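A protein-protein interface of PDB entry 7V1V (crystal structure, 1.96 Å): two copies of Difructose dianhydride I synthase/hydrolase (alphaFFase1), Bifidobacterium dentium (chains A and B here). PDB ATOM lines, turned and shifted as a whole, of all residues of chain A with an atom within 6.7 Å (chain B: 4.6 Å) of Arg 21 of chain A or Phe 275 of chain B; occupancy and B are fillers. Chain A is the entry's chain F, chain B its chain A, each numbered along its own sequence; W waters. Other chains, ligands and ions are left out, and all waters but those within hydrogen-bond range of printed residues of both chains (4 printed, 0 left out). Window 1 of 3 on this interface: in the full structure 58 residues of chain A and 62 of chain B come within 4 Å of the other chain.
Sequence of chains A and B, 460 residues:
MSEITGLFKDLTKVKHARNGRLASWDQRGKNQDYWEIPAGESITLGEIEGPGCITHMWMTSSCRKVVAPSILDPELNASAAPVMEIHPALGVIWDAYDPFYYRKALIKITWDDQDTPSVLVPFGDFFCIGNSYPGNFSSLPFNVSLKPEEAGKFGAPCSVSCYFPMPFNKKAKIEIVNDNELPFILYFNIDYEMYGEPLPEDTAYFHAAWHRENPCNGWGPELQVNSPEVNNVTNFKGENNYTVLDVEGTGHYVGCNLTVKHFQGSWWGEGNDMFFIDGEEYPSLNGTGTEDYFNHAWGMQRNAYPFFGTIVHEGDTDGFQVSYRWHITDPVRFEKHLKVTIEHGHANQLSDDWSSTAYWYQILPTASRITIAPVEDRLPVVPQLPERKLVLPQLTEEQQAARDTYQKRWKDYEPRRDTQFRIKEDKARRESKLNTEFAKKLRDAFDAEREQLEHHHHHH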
ATOM      1  N   ASN A  19     -14.298   7.724  -4.162  1.00  0.00           N
ATOM      2  CA  ASN A  19     -14.631   8.343  -5.473  1.00  0.00           C
ATOM      3  C   ASN A  19     -15.772   7.554  -6.126  1.00  0.00           C
ATOM      4  O   ASN A  19     -15.796   6.338  -5.988  1.00  0.00           O
ATOM      5  CB  ASN A  19     -13.429   8.389  -6.414  1.00  0.00           C
ATOM      6  CG  ASN A  19     -12.520   9.557  -6.104  1.00  0.00           C
ATOM      7  OD1 ASN A  19     -12.539  10.588  -6.802  1.00  0.00           O
ATOM      8  ND2 ASN A  19     -11.779   9.436  -5.022  1.00  0.00           N
ATOM      9  N   GLY A  20     -16.668   8.266  -6.802  1.00  0.00           N
ATOM     10  CA  GLY A  20     -17.611   7.716  -7.776  1.00  0.00           C
ATOM     11  C   GLY A  20     -17.730   8.639  -8.964  1.00  0.00           C
ATOM     12  O   GLY A  20     -17.219   9.793  -8.899  1.00  0.00           O
ATOM     13  N   ARG A  21     -18.325   8.148 -10.037  1.00  0.00           N
ATOM     14  CA  ARG A  21     -18.512   8.955 -11.263  1.00  0.00           C
ATOM     15  C   ARG A  21     -19.784   8.525 -11.997  1.00  0.00           C
ATOM     16  O   ARG A  21     -19.920   7.324 -12.303  1.00  0.00           O
ATOM     17  CB  ARG A  21     -17.278   8.821 -12.150  1.00  0.00           C
ATOM     18  CG  ARG A  21     -17.320   9.706 -13.382  1.00  0.00           C
ATOM     19  CD  ARG A  21     -16.209   9.353 -14.324  1.00  0.00           C
ATOM     20  NE  ARG A  21     -14.869   9.683 -13.822  1.00  0.00           N
ATOM     21  CZ  ARG A  21     -13.776   9.147 -14.342  1.00  0.00           C
ATOM     22  NH1 ARG A  21     -13.888   8.292 -15.345  1.00  0.00           N
ATOM     23  NH2 ARG A  21     -12.581   9.437 -13.868  1.00  0.00           N
ATOM     24  N   LEU A  22     -20.672   9.478 -12.284  1.00  0.00           N
ATOM     25  CA  LEU A  22     -21.748   9.285 -13.304  1.00  0.00           C
ATOM     26  C   LEU A  22     -21.196   9.689 -14.672  1.00  0.00           C
ATOM     27  O   LEU A  22     -20.775  10.849 -14.841  1.00  0.00           O
ATOM     28  CB  LEU A  22     -22.961  10.151 -12.984  1.00  0.00           C
ATOM     29  CG  LEU A  22     -23.475  10.112 -11.553  1.00  0.00           C
ATOM     30  CD1 LEU A  22     -24.601  11.108 -11.374  1.00  0.00           C
ATOM     31  CD2 LEU A  22     -23.927   8.710 -11.196  1.00  0.00           C
ATOM     32  N   ALA A  23     -21.213   8.773 -15.627  1.00  0.00           N
ATOM     33  CA  ALA A  23     -20.661   8.997 -16.975  1.00  0.00           C
ATOM     34  C   ALA A  23     -21.617   8.377 -17.991  1.00  0.00           C
ATOM     35  O   ALA A  23     -22.462   7.468 -17.610  1.00  0.00           O
ATOM     36  CB  ALA A  23     -19.257   8.421 -17.063  1.00  0.00           C
ATOM     37  N   TRP A  25     -20.540   6.527 -20.228  1.00  0.00           N
ATOM     38  CA  TRP A  25     -19.765   5.377 -20.744  1.00  0.00           C
ATOM     39  C   TRP A  25     -20.699   4.335 -21.361  1.00  0.00           C
ATOM     40  O   TRP A  25     -21.825   4.181 -20.901  1.00  0.00           O
ATOM     41  CB  TRP A  25     -18.828   4.780 -19.701  1.00  0.00           C
ATOM     42  CG  TRP A  25     -19.480   4.033 -18.573  1.00  0.00           C
ATOM     43  CD1 TRP A  25     -20.155   4.556 -17.517  1.00  0.00           C
ATOM     44  CD2 TRP A  25     -19.413   2.618 -18.344  1.00  0.00           C
ATOM     45  NE1 TRP A  25     -20.512   3.572 -16.639  1.00  0.00           N
ATOM     46  CE2 TRP A  25     -20.077   2.365 -17.123  1.00  0.00           C
ATOM     47  CE3 TRP A  25     -18.869   1.543 -19.055  1.00  0.00           C
ATOM     48  CZ2 TRP A  25     -20.236   1.071 -16.617  1.00  0.00           C
ATOM     49  CZ3 TRP A  25     -19.015   0.266 -18.557  1.00  0.00           C
ATOM     50  CH2 TRP A  25     -19.660   0.043 -17.334  1.00  0.00           C
ATOM     51  N   ILE A  48     -27.456   9.942  -6.631  1.00  0.00           N
ATOM     52  CA  ILE A  48     -26.390   9.499  -5.689  1.00  0.00           C
ATOM     53  C   ILE A  48     -26.949   9.677  -4.281  1.00  0.00           C
ATOM     54  O   ILE A  48     -27.475  10.790  -3.985  1.00  0.00           O
ATOM     55  CB  ILE A  48     -25.095  10.317  -5.905  1.00  0.00           C
ATOM     56  CG1 ILE A  48     -24.634  10.302  -7.370  1.00  0.00           C
ATOM     57  CG2 ILE A  48     -23.993   9.879  -4.943  1.00  0.00           C
ATOM     58  CD1 ILE A  48     -23.899  11.568  -7.763  1.00  0.00           C
ATOM     59  N   HIS A  56     -16.486  17.700  -9.754  1.00  0.00           N
ATOM     60  CA  HIS A  56     -16.133  18.033 -11.150  1.00  0.00           C
ATOM     61  C   HIS A  56     -17.223  17.537 -12.098  1.00  0.00           C
ATOM     62  O   HIS A  56     -17.664  16.390 -11.969  1.00  0.00           O
ATOM     63  CB  HIS A  56     -14.766  17.444 -11.509  1.00  0.00           C
ATOM     64  CG  HIS A  56     -14.548  17.210 -12.966  1.00  0.00           C
ATOM     65  ND1 HIS A  56     -14.173  18.221 -13.853  1.00  0.00           N
ATOM     66  CD2 HIS A  56     -14.627  16.087 -13.706  1.00  0.00           C
ATOM     67  CE1 HIS A  56     -14.009  17.698 -15.061  1.00  0.00           C
ATOM     68  NE2 HIS A  56     -14.311  16.410 -14.995  1.00  0.00           N
ATOM     69  N   PHE A 188     -20.885  12.874 -20.843  1.00  0.00           N
ATOM     70  CA  PHE A 188     -20.671  13.513 -19.523  1.00  0.00           C
ATOM     71  C   PHE A 188     -19.766  12.631 -18.659  1.00  0.00           C
ATOM     72  O   PHE A 188     -19.736  11.403 -18.813  1.00  0.00           O
ATOM     73  CB  PHE A 188     -22.016  13.887 -18.882  1.00  0.00           C
ATOM     74  CG  PHE A 188     -22.901  12.712 -18.521  1.00  0.00           C
ATOM     75  CD1 PHE A 188     -23.815  12.199 -19.429  1.00  0.00           C
ATOM     76  CD2 PHE A 188     -22.839  12.134 -17.259  1.00  0.00           C
ATOM     77  CE1 PHE A 188     -24.659  11.146 -19.081  1.00  0.00           C
ATOM     78  CE2 PHE A 188     -23.650  11.052 -16.919  1.00  0.00           C
ATOM     79  CZ  PHE A 188     -24.588  10.582 -17.819  1.00  0.00           C
ATOM     80  N   ASN A 189     -19.046  13.290 -17.754  1.00  0.00           N
ATOM     81  CA  ASN A 189     -18.381  12.662 -16.587  1.00  0.00           C
ATOM     82  C   ASN A 189     -18.678  13.571 -15.389  1.00  0.00           C
ATOM     83  O   ASN A 189     -18.278  14.750 -15.429  1.00  0.00           O
ATOM     84  CB  ASN A 189     -16.863  12.556 -16.707  1.00  0.00           C
ATOM     85  CG  ASN A 189     -16.257  11.932 -17.940  1.00  0.00           C
ATOM     86  OD1 ASN A 189     -16.901  11.285 -18.776  1.00  0.00           O
ATOM     87  ND2 ASN A 189     -14.955  12.113 -18.037  1.00  0.00           N
ATOM     88  N   ILE A 190     -19.395  13.076 -14.385  1.00  0.00           N
ATOM     89  CA  ILE A 190     -19.700  13.816 -13.133  1.00  0.00           C
ATOM     90  C   ILE A 190     -19.038  13.089 -11.969  1.00  0.00           C
ATOM     91  O   ILE A 190     -19.484  11.992 -11.610  1.00  0.00           O
ATOM     92  CB  ILE A 190     -21.215  13.964 -12.938  1.00  0.00           C
ATOM     93  CG1 ILE A 190     -21.866  14.646 -14.152  1.00  0.00           C
ATOM     94  CG2 ILE A 190     -21.500  14.725 -11.651  1.00  0.00           C
ATOM     95  CD1 ILE A 190     -23.362  14.453 -14.231  1.00  0.00           C
ATOM     96  N   ASP A 191     -17.998  13.704 -11.418  1.00  0.00           N
ATOM     97  CA  ASP A 191     -17.124  13.109 -10.397  1.00  0.00           C
ATOM     98  C   ASP A 191     -17.618  13.600  -9.043  1.00  0.00           C
ATOM     99  O   ASP A 191     -18.084  14.767  -8.919  1.00  0.00           O
ATOM    100  CB  ASP A 191     -15.671  13.462 -10.691  1.00  0.00           C
ATOM    101  CG  ASP A 191     -15.183  12.749 -11.931  1.00  0.00           C
ATOM    102  OD1 ASP A 191     -14.750  11.604 -11.766  1.00  0.00           O
ATOM    103  OD2 ASP A 191     -15.298  13.331 -13.057  1.00  0.00           O
ATOM    104  N   TYR A 192     -17.508  12.726  -8.069  1.00  0.00           N
ATOM    105  CA  TYR A 192     -18.038  12.987  -6.726  1.00  0.00           C
ATOM    106  C   TYR A 192     -17.243  12.120  -5.773  1.00  0.00           C
ATOM    107  O   TYR A 192     -16.521  11.222  -6.229  1.00  0.00           O
ATOM    108  CB  TYR A 192     -19.549  12.751  -6.692  1.00  0.00           C
ATOM    109  CG  TYR A 192     -20.032  11.339  -6.921  1.00  0.00           C
ATOM    110  CD1 TYR A 192     -20.163  10.437  -5.866  1.00  0.00           C
ATOM    111  CD2 TYR A 192     -20.460  10.930  -8.171  1.00  0.00           C
ATOM    112  CE1 TYR A 192     -20.689   9.162  -6.064  1.00  0.00           C
ATOM    113  CE2 TYR A 192     -20.947   9.646  -8.385  1.00  0.00           C
ATOM    114  CZ  TYR A 192     -21.085   8.759  -7.330  1.00  0.00           C
ATOM    115  OH  TYR A 192     -21.579   7.499  -7.576  1.00  0.00           O
ATOM    116  N   ASN A 435     -26.732   3.604 -14.299  1.00  0.00           N
ATOM    117  CA  ASN A 435     -25.877   4.587 -13.581  1.00  0.00           C
ATOM    118  C   ASN A 435     -26.284   4.681 -12.112  1.00  0.00           C
ATOM    119  O   ASN A 435     -25.384   4.665 -11.261  1.00  0.00           O
ATOM    120  CB  ASN A 435     -25.923   5.983 -14.207  1.00  0.00           C
ATOM    121  CG  ASN A 435     -24.898   6.159 -15.299  1.00  0.00           C
ATOM    122  OD1 ASN A 435     -24.236   5.207 -15.713  1.00  0.00           O
ATOM    123  ND2 ASN A 435     -24.798   7.378 -15.800  1.00  0.00           N
ATOM    124  N   PHE A 438     -25.557   1.366 -10.131  1.00  0.00           N
ATOM    125  CA  PHE A 438     -24.116   1.203  -9.803  1.00  0.00           C
ATOM    126  C   PHE A 438     -23.756   2.153  -8.657  1.00  0.00           C
ATOM    127  O   PHE A 438     -23.034   1.734  -7.689  1.00  0.00           O
ATOM    128  CB  PHE A 438     -23.224   1.394 -11.029  1.00  0.00           C
ATOM    129  CG  PHE A 438     -21.769   1.093 -10.750  1.00  0.00           C
ATOM    130  CD1 PHE A 438     -21.305  -0.215 -10.728  1.00  0.00           C
ATOM    131  CD2 PHE A 438     -20.888   2.110 -10.430  1.00  0.00           C
ATOM    132  CE1 PHE A 438     -19.971  -0.489 -10.454  1.00  0.00           C
ATOM    133  CE2 PHE A 438     -19.559   1.836 -10.150  1.00  0.00           C
ATOM    134  CZ  PHE A 438     -19.100   0.538 -10.158  1.00  0.00           C
ATOM    135  N   ALA A 439     -24.248   3.392  -8.718  1.00  0.00           N
ATOM    136  CA  ALA A 439     -23.964   4.420  -7.679  1.00  0.00           C
ATOM    137  C   ALA A 439     -24.429   3.897  -6.314  1.00  0.00           C
ATOM    138  O   ALA A 439     -23.741   4.145  -5.291  1.00  0.00           O
ATOM    139  CB  ALA A 439     -24.626   5.730  -8.033  1.00  0.00           C
ATOM    140  N   LEU A 442     -22.135   1.016  -5.111  1.00  0.00           N
ATOM    141  CA  LEU A 442     -20.864   1.640  -4.684  1.00  0.00           C
ATOM    142  C   LEU A 442     -21.057   2.247  -3.295  1.00  0.00           C
ATOM    143  O   LEU A 442     -20.191   2.035  -2.413  1.00  0.00           O
ATOM    144  CB  LEU A 442     -20.498   2.688  -5.748  1.00  0.00           C
ATOM    145  CG  LEU A 442     -19.024   2.995  -5.953  1.00  0.00           C
ATOM    146  CD1 LEU A 442     -18.217   1.753  -6.280  1.00  0.00           C
ATOM    147  CD2 LEU A 442     -18.883   4.036  -7.071  1.00  0.00           C
ATOM    148  N   TYR B 253      -4.459  10.256  -6.226  1.00  0.00           N
ATOM    149  CA  TYR B 253      -3.873  10.640  -7.527  1.00  0.00           C
ATOM    150  C   TYR B 253      -4.248  12.100  -7.785  1.00  0.00           C
ATOM    151  O   TYR B 253      -5.435  12.475  -7.597  1.00  0.00           O
ATOM    152  CB  TYR B 253      -4.448   9.689  -8.552  1.00  0.00           C
ATOM    153  CG  TYR B 253      -4.303  10.088  -9.994  1.00  0.00           C
ATOM    154  CD1 TYR B 253      -3.092   9.984 -10.650  1.00  0.00           C
ATOM    155  CD2 TYR B 253      -5.407  10.484 -10.715  1.00  0.00           C
ATOM    156  CE1 TYR B 253      -2.976  10.238 -12.011  1.00  0.00           C
ATOM    157  CE2 TYR B 253      -5.313  10.751 -12.077  1.00  0.00           C
ATOM    158  CZ  TYR B 253      -4.091  10.652 -12.714  1.00  0.00           C
ATOM    159  OH  TYR B 253      -4.036  10.907 -14.036  1.00  0.00           O
ATOM    160  N   ASP B 273     -10.569   6.561 -20.035  1.00  0.00           N
ATOM    161  CA  ASP B 273      -9.963   6.395 -18.699  1.00  0.00           C
ATOM    162  C   ASP B 273     -10.774   5.332 -17.952  1.00  0.00           C
ATOM    163  O   ASP B 273     -12.012   5.338 -18.018  1.00  0.00           O
ATOM    164  CB  ASP B 273      -9.863   7.728 -17.963  1.00  0.00           C
ATOM    165  CG  ASP B 273     -11.147   8.514 -17.858  1.00  0.00           C
ATOM    166  OD1 ASP B 273     -11.706   8.864 -18.904  1.00  0.00           O
ATOM    167  OD2 ASP B 273     -11.546   8.793 -16.720  1.00  0.00           O
ATOM    168  N   MET B 274     -10.083   4.476 -17.219  1.00  0.00           N
ATOM    169  CA  MET B 274     -10.704   3.483 -16.317  1.00  0.00           C
ATOM    170  C   MET B 274      -9.851   3.417 -15.055  1.00  0.00           C
ATOM    171  O   MET B 274      -8.647   3.072 -15.177  1.00  0.00           O
ATOM    172  CB  MET B 274     -10.782   2.119 -16.999  1.00  0.00           C
ATOM    173  CG  MET B 274     -11.697   2.100 -18.203  1.00  0.00           C
ATOM    174  SD  MET B 274     -11.849   0.443 -18.881  1.00  0.00           S
ATOM    175  CE  MET B 274     -12.781   0.760 -20.375  1.00  0.00           C
ATOM    176  N   PHE B 275     -10.459   3.787 -13.928  1.00  0.00           N
ATOM    177  CA  PHE B 275      -9.819   3.797 -12.590  1.00  0.00           C
ATOM    178  C   PHE B 275     -10.302   2.596 -11.783  1.00  0.00           C
ATOM    179  O   PHE B 275     -11.523   2.350 -11.700  1.00  0.00           O
ATOM    180  CB  PHE B 275     -10.119   5.090 -11.846  1.00  0.00           C
ATOM    181  CG  PHE B 275      -9.480   6.319 -12.441  1.00  0.00           C
ATOM    182  CD1 PHE B 275     -10.023   6.941 -13.560  1.00  0.00           C
ATOM    183  CD2 PHE B 275      -8.368   6.885 -11.849  1.00  0.00           C
ATOM    184  CE1 PHE B 275      -9.466   8.113 -14.051  1.00  0.00           C
ATOM    185  CE2 PHE B 275      -7.808   8.047 -12.350  1.00  0.00           C
ATOM    186  CZ  PHE B 275      -8.347   8.642 -13.461  1.00  0.00           C
ATOM    187  N   PHE B 276      -9.344   1.854 -11.251  1.00  0.00           N
ATOM    188  CA  PHE B 276      -9.574   0.671 -10.383  1.00  0.00           C
ATOM    189  C   PHE B 276      -9.137   1.037  -8.982  1.00  0.00           C
ATOM    190  O   PHE B 276      -7.912   1.225  -8.761  1.00  0.00           O
ATOM    191  CB  PHE B 276      -8.776  -0.527 -10.864  1.00  0.00           C
ATOM    192  CG  PHE B 276      -9.064  -0.919 -12.289  1.00  0.00           C
ATOM    193  CD1 PHE B 276      -8.554  -0.167 -13.346  1.00  0.00           C
ATOM    194  CD2 PHE B 276      -9.829  -2.041 -12.570  1.00  0.00           C
ATOM    195  CE1 PHE B 276      -8.779  -0.566 -14.653  1.00  0.00           C
ATOM    196  CE2 PHE B 276     -10.087  -2.406 -13.883  1.00  0.00           C
ATOM    197  CZ  PHE B 276      -9.554  -1.670 -14.921  1.00  0.00           C
ATOM    198  N   ILE B 277     -10.116   1.191  -8.093  1.00  0.00           N
ATOM    199  CA  ILE B 277      -9.863   1.600  -6.691  1.00  0.00           C
ATOM    200  C   ILE B 277      -9.920   0.369  -5.769  1.00  0.00           C
ATOM    201  O   ILE B 277     -10.917  -0.396  -5.830  1.00  0.00           O
ATOM    202  CB  ILE B 277     -10.849   2.703  -6.299  1.00  0.00           C
ATOM    203  CG1 ILE B 277     -10.585   3.970  -7.127  1.00  0.00           C
ATOM    204  CG2 ILE B 277     -10.807   2.944  -4.800  1.00  0.00           C
ATOM    205  CD1 ILE B 277     -11.703   4.970  -7.102  1.00  0.00           C
ATOM    206  N   GLU B 280     -10.587  -3.511  -6.788  1.00  0.00           N
ATOM    207  CA  GLU B 280     -11.803  -3.943  -7.532  1.00  0.00           C
ATOM    208  C   GLU B 280     -11.389  -4.519  -8.894  1.00  0.00           C
ATOM    209  O   GLU B 280     -10.392  -4.053  -9.510  1.00  0.00           O
ATOM    210  CB  GLU B 280     -12.820  -2.812  -7.679  1.00  0.00           C
ATOM    211  CG  GLU B 280     -12.298  -1.596  -8.439  1.00  0.00           C
ATOM    212  CD  GLU B 280     -13.174  -0.350  -8.326  1.00  0.00           C
ATOM    213  OE1 GLU B 280     -14.270  -0.400  -7.681  1.00  0.00           O
ATOM    214  OE2 GLU B 280     -12.759   0.686  -8.877  1.00  0.00           O
ATOM    215  N   PRO B 283     -13.498  -1.536 -13.256  1.00  0.00           N
ATOM    216  CA  PRO B 283     -13.274  -0.145 -12.871  1.00  0.00           C
ATOM    217  C   PRO B 283     -14.573   0.452 -12.326  1.00  0.00           C
ATOM    218  O   PRO B 283     -15.578   0.347 -12.978  1.00  0.00           O
ATOM    219  CB  PRO B 283     -12.786   0.532 -14.187  1.00  0.00           C
ATOM    220  CG  PRO B 283     -13.333  -0.343 -15.290  1.00  0.00           C
ATOM    221  CD  PRO B 283     -13.348  -1.752 -14.711  1.00  0.00           C
ATOM    222  N   SER B 284     -14.509   1.119 -11.180  1.00  0.00           N
ATOM    223  CA  SER B 284     -15.630   1.907 -10.618  1.00  0.00           C
ATOM    224  C   SER B 284     -15.764   3.274 -11.316  1.00  0.00           C
ATOM    225  O   SER B 284     -16.883   3.805 -11.324  1.00  0.00           O
ATOM    226  CB  SER B 284     -15.516   2.050  -9.129  1.00  0.00           C
ATOM    227  OG  SER B 284     -14.280   2.626  -8.736  1.00  0.00           O
ATOM    228  N   LEU B 285     -14.663   3.849 -11.808  1.00  0.00           N
ATOM    229  CA  LEU B 285     -14.648   5.159 -12.522  1.00  0.00           C
ATOM    230  C   LEU B 285     -14.440   4.872 -14.002  1.00  0.00           C
ATOM    231  O   LEU B 285     -13.305   4.509 -14.370  1.00  0.00           O
ATOM    232  CB  LEU B 285     -13.506   6.046 -12.019  1.00  0.00           C
ATOM    233  CG  LEU B 285     -13.738   6.875 -10.749  1.00  0.00           C
ATOM    234  CD1 LEU B 285     -14.669   6.233  -9.756  1.00  0.00           C
ATOM    235  CD2 LEU B 285     -12.422   7.228 -10.084  1.00  0.00           C
ATOM    236  N   ASN B 286     -15.485   5.069 -14.796  1.00  0.00           N
ATOM    237  CA  ASN B 286     -15.478   4.834 -16.252  1.00  0.00           C
ATOM    238  C   ASN B 286     -15.572   6.171 -16.976  1.00  0.00           C
ATOM    239  O   ASN B 286     -16.551   6.949 -16.714  1.00  0.00           O
ATOM    240  CB  ASN B 286     -16.615   3.917 -16.720  1.00  0.00           C
ATOM    241  CG  ASN B 286     -16.293   2.455 -16.506  1.00  0.00           C
ATOM    242  OD1 ASN B 286     -15.444   1.886 -17.193  1.00  0.00           O
ATOM    243  ND2 ASN B 286     -16.911   1.862 -15.491  1.00  0.00           N
ATOM    244  N   GLY B 287     -14.573   6.437 -17.824  1.00  0.00           N
ATOM    245  CA  GLY B 287     -14.576   7.626 -18.692  1.00  0.00           C
ATOM    246  C   GLY B 287     -15.214   7.308 -20.022  1.00  0.00           C
ATOM    247  O   GLY B 287     -15.741   6.173 -20.184  1.00  0.00           O
ATOM    248  N   TYR B 293     -11.192  12.795 -21.009  1.00  0.00           N
ATOM    249  CA  TYR B 293     -10.424  12.761 -19.729  1.00  0.00           C
ATOM    250  C   TYR B 293      -9.685  14.105 -19.508  1.00  0.00           C
ATOM    251  O   TYR B 293      -9.726  14.711 -18.389  1.00  0.00           O
ATOM    252  CB  TYR B 293      -9.472  11.562 -19.684  1.00  0.00           C
ATOM    253  CG  TYR B 293      -8.562  11.608 -18.489  1.00  0.00           C
ATOM    254  CD1 TYR B 293      -9.089  11.468 -17.221  1.00  0.00           C
ATOM    255  CD2 TYR B 293      -7.216  11.926 -18.604  1.00  0.00           C
ATOM    256  CE1 TYR B 293      -8.307  11.591 -16.092  1.00  0.00           C
ATOM    257  CE2 TYR B 293      -6.403  12.005 -17.485  1.00  0.00           C
ATOM    258  CZ  TYR B 293      -6.965  11.889 -16.218  1.00  0.00           C
ATOM    259  OH  TYR B 293      -6.212  11.985 -15.079  1.00  0.00           O
ATOM    260  N   VAL B 332      -8.380  11.634  -7.041  1.00  0.00           N
ATOM    261  CA  VAL B 332      -8.884  10.234  -7.002  1.00  0.00           C
ATOM    262  C   VAL B 332      -8.185   9.536  -5.830  1.00  0.00           C
ATOM    263  O   VAL B 332      -6.975   9.240  -5.949  1.00  0.00           O
ATOM    264  CB  VAL B 332      -8.666   9.504  -8.332  1.00  0.00           C
ATOM    265  CG1 VAL B 332      -9.305   8.123  -8.297  1.00  0.00           C
ATOM    266  CG2 VAL B 332      -9.201  10.332  -9.494  1.00  0.00           C
ATOM    267  N   LEU B 338      -4.459   1.875  -6.068  1.00  0.00           N
ATOM    268  CA  LEU B 338      -5.054   2.610  -7.209  1.00  0.00           C
ATOM    269  C   LEU B 338      -4.362   2.147  -8.465  1.00  0.00           C
ATOM    270  O   LEU B 338      -3.116   2.135  -8.510  1.00  0.00           O
ATOM    271  CB  LEU B 338      -4.897   4.127  -7.056  1.00  0.00           C
ATOM    272  CG  LEU B 338      -5.454   4.928  -8.228  1.00  0.00           C
ATOM    273  CD1 LEU B 338      -6.953   4.677  -8.348  1.00  0.00           C
ATOM    274  CD2 LEU B 338      -5.164   6.412  -8.079  1.00  0.00           C
ATOM    275  N   LYS B 339      -5.163   1.834  -9.463  1.00  0.00           N
ATOM    276  CA  LYS B 339      -4.658   1.637 -10.826  1.00  0.00           C
ATOM    277  C   LYS B 339      -5.324   2.665 -11.729  1.00  0.00           C
ATOM    278  O   LYS B 339      -6.546   2.623 -11.835  1.00  0.00           O
ATOM    279  CB  LYS B 339      -4.968   0.249 -11.358  1.00  0.00           C
ATOM    280  CG  LYS B 339      -4.102  -0.100 -12.552  1.00  0.00           C
ATOM    281  CD  LYS B 339      -4.431  -1.471 -13.121  1.00  0.00           C
ATOM    282  CE  LYS B 339      -3.365  -1.917 -14.093  1.00  0.00           C
ATOM    283  NZ  LYS B 339      -3.673  -3.252 -14.653  1.00  0.00           N
ATOM    284  N   VAL B 340      -4.529   3.496 -12.396  1.00  0.00           N
ATOM    285  CA  VAL B 340      -5.031   4.539 -13.338  1.00  0.00           C
ATOM    286  C   VAL B 340      -4.699   4.057 -14.749  1.00  0.00           C
ATOM    287  O   VAL B 340      -3.489   3.845 -15.043  1.00  0.00           O
ATOM    288  CB  VAL B 340      -4.385   5.911 -13.053  1.00  0.00           C
ATOM    289  CG1 VAL B 340      -4.915   6.965 -14.020  1.00  0.00           C
ATOM    290  CG2 VAL B 340      -4.581   6.365 -11.613  1.00  0.00           C
HETATM  291  O   HOH W   1     -12.865  11.102 -16.572  1.00  0.00           O
HETATM  292  O   HOH W   2     -18.218   5.634 -13.821  1.00  0.00           O
HETATM  293  O   HOH W   3     -18.819   5.345 -10.439  1.00  0.00           O
HETATM  294  O   HOH W   4     -13.465  10.423 -19.997  1.00  0.00           O
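No position is printed for both chains.
Of the 14 pairs that touch across the chains among the printed residues, none has its exchanged pair printed and touching as well.
Of the 17 printed residues of chain B, 8 touch a printed residue of chain A.
Hydrophobic or aromatic side chains of chain B that line the printed part of chain A: Phe 275, Ile 277 and Leu 285.
Printed residues of chain A that touch a printed residue of chain B: Asn 19, Gly 20, Arg 21, Ala 23, Trp 25, Phe 438 and Leu 442.
Hydrophobic or aromatic side chains of chain A within 4 Å of the printed part of chain B: Ala 23, Trp 25, Phe 438 and Leu 442.
Among the printed residues, Asp or Glu carboxylates within 4 Å of a Lys or Arg side-chain nitrogen of the other chain: Arg 21 of chain A with Asp 273 of chain B (2.8 Å).
Water W4 lies within hydrogen-bond range of OD1 of Asp 273 of chain B (2.6 Å), ND2 of Asn 189 of chain A (3.0 Å) and N of Tyr 293 of chain B (3.4 Å).
Water W1 lies within hydrogen-bond range of OD2 of Asp 273 of chain B (2.7 Å), ND2 of Asn 189 of chain A (2.7 Å) and NH2 of Arg 21 of chain A (3.2 Å).
Water W2 lies within hydrogen-bond range of O of Arg 21 of chain A (2.8 Å), N of Asn 286 of chain B (3.0 Å) and O of Ser 284 of chain B (3.4 Å).
CD1 of Leu 285 of chain B touches O of Asn 19 of chain A (3.9 Å).
ND2 of Asn 19 of chain A touches CA of Val 332 of chain B, at 3.6 Å.
Gly 20 of chain A touches Leu 285 of chain B (CA to CD1, 3.8 Å).
Arg 21 of chain A touches Phe 275 of chain B (NH2 to CE1, 3.4 Å).
NH1 of Arg 21 of chain A touches C of Leu 285 of chain B, 3.7 Å away.
Asn 286 of chain B touches Ala 23 of chain A (O to CB, 3.1 Å).
Trp 25 of chain A touches Asn 286 of chain B (CG to CB, 3.4 Å).
CD1 of Leu 442 of chain A touches CB of Ser 284 of chain B (3.9 Å).
The side-chain carboxylate (OD2) of Asp 273 of chain B is in salt-bridge range of the guanidinium group (NH1) of Arg 21 of chain A (2.8 Å).
NH1 of Arg 21 of chain A sits close to N of Gly 287 of chain B (3.2 Å).
The backbone carbonyl oxygen of Asn 286 of chain B sits close to the guanidinium group of Arg 21 of chain A (3.3 Å).
Of the printed residues of chain B, Asn 19 of chain A touches Ile 277, Leu 285 and Val 332.
Of chain B, only Asp 273 (2.8 Å), Phe 275 (3.4 Å), Leu 285 (3.7 Å), Asn 286 (3.2 Å) and Gly 287 (3.2 Å) come within 4 Å of Arg 21 of chain A.
Of the printed residues of chain B, Leu 442 of chain A touches Ser 284 (3.9 Å).
Printed residues of chain A within 4 Å of Ser 284 of chain B: Phe 438 (3.5 Å) and Leu 442 (3.9 Å).
Printed residues of chain A within 4 Å of Val 332 of chain B: Asn 19 (3.6 Å).
The nearest printed residue of chain A that does not touch Phe 275 of chain B is Asp 191 of chain A (6.7 Å).
N of Ile 277 of chain B lies within hydrogen-bond range of OE2 of Glu 280 of chain B, 2.8 Å away.
N of Phe 275 of chain B sits at hydrogen-bond distance from O of Leu 285 of chain B, 3.0 Å away.
OE2 of Glu 280 of chain B sits at hydrogen-bond distance from OG of Ser 284 of chain B.
O of Ala 23 of chain A lies within hydrogen-bond range of ND2 of Asn 435 of chain A (3.0 Å).
O of Tyr 192 of chain A lies within hydrogen-bond range of N of Gly 20 of chain A (3.0 Å).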
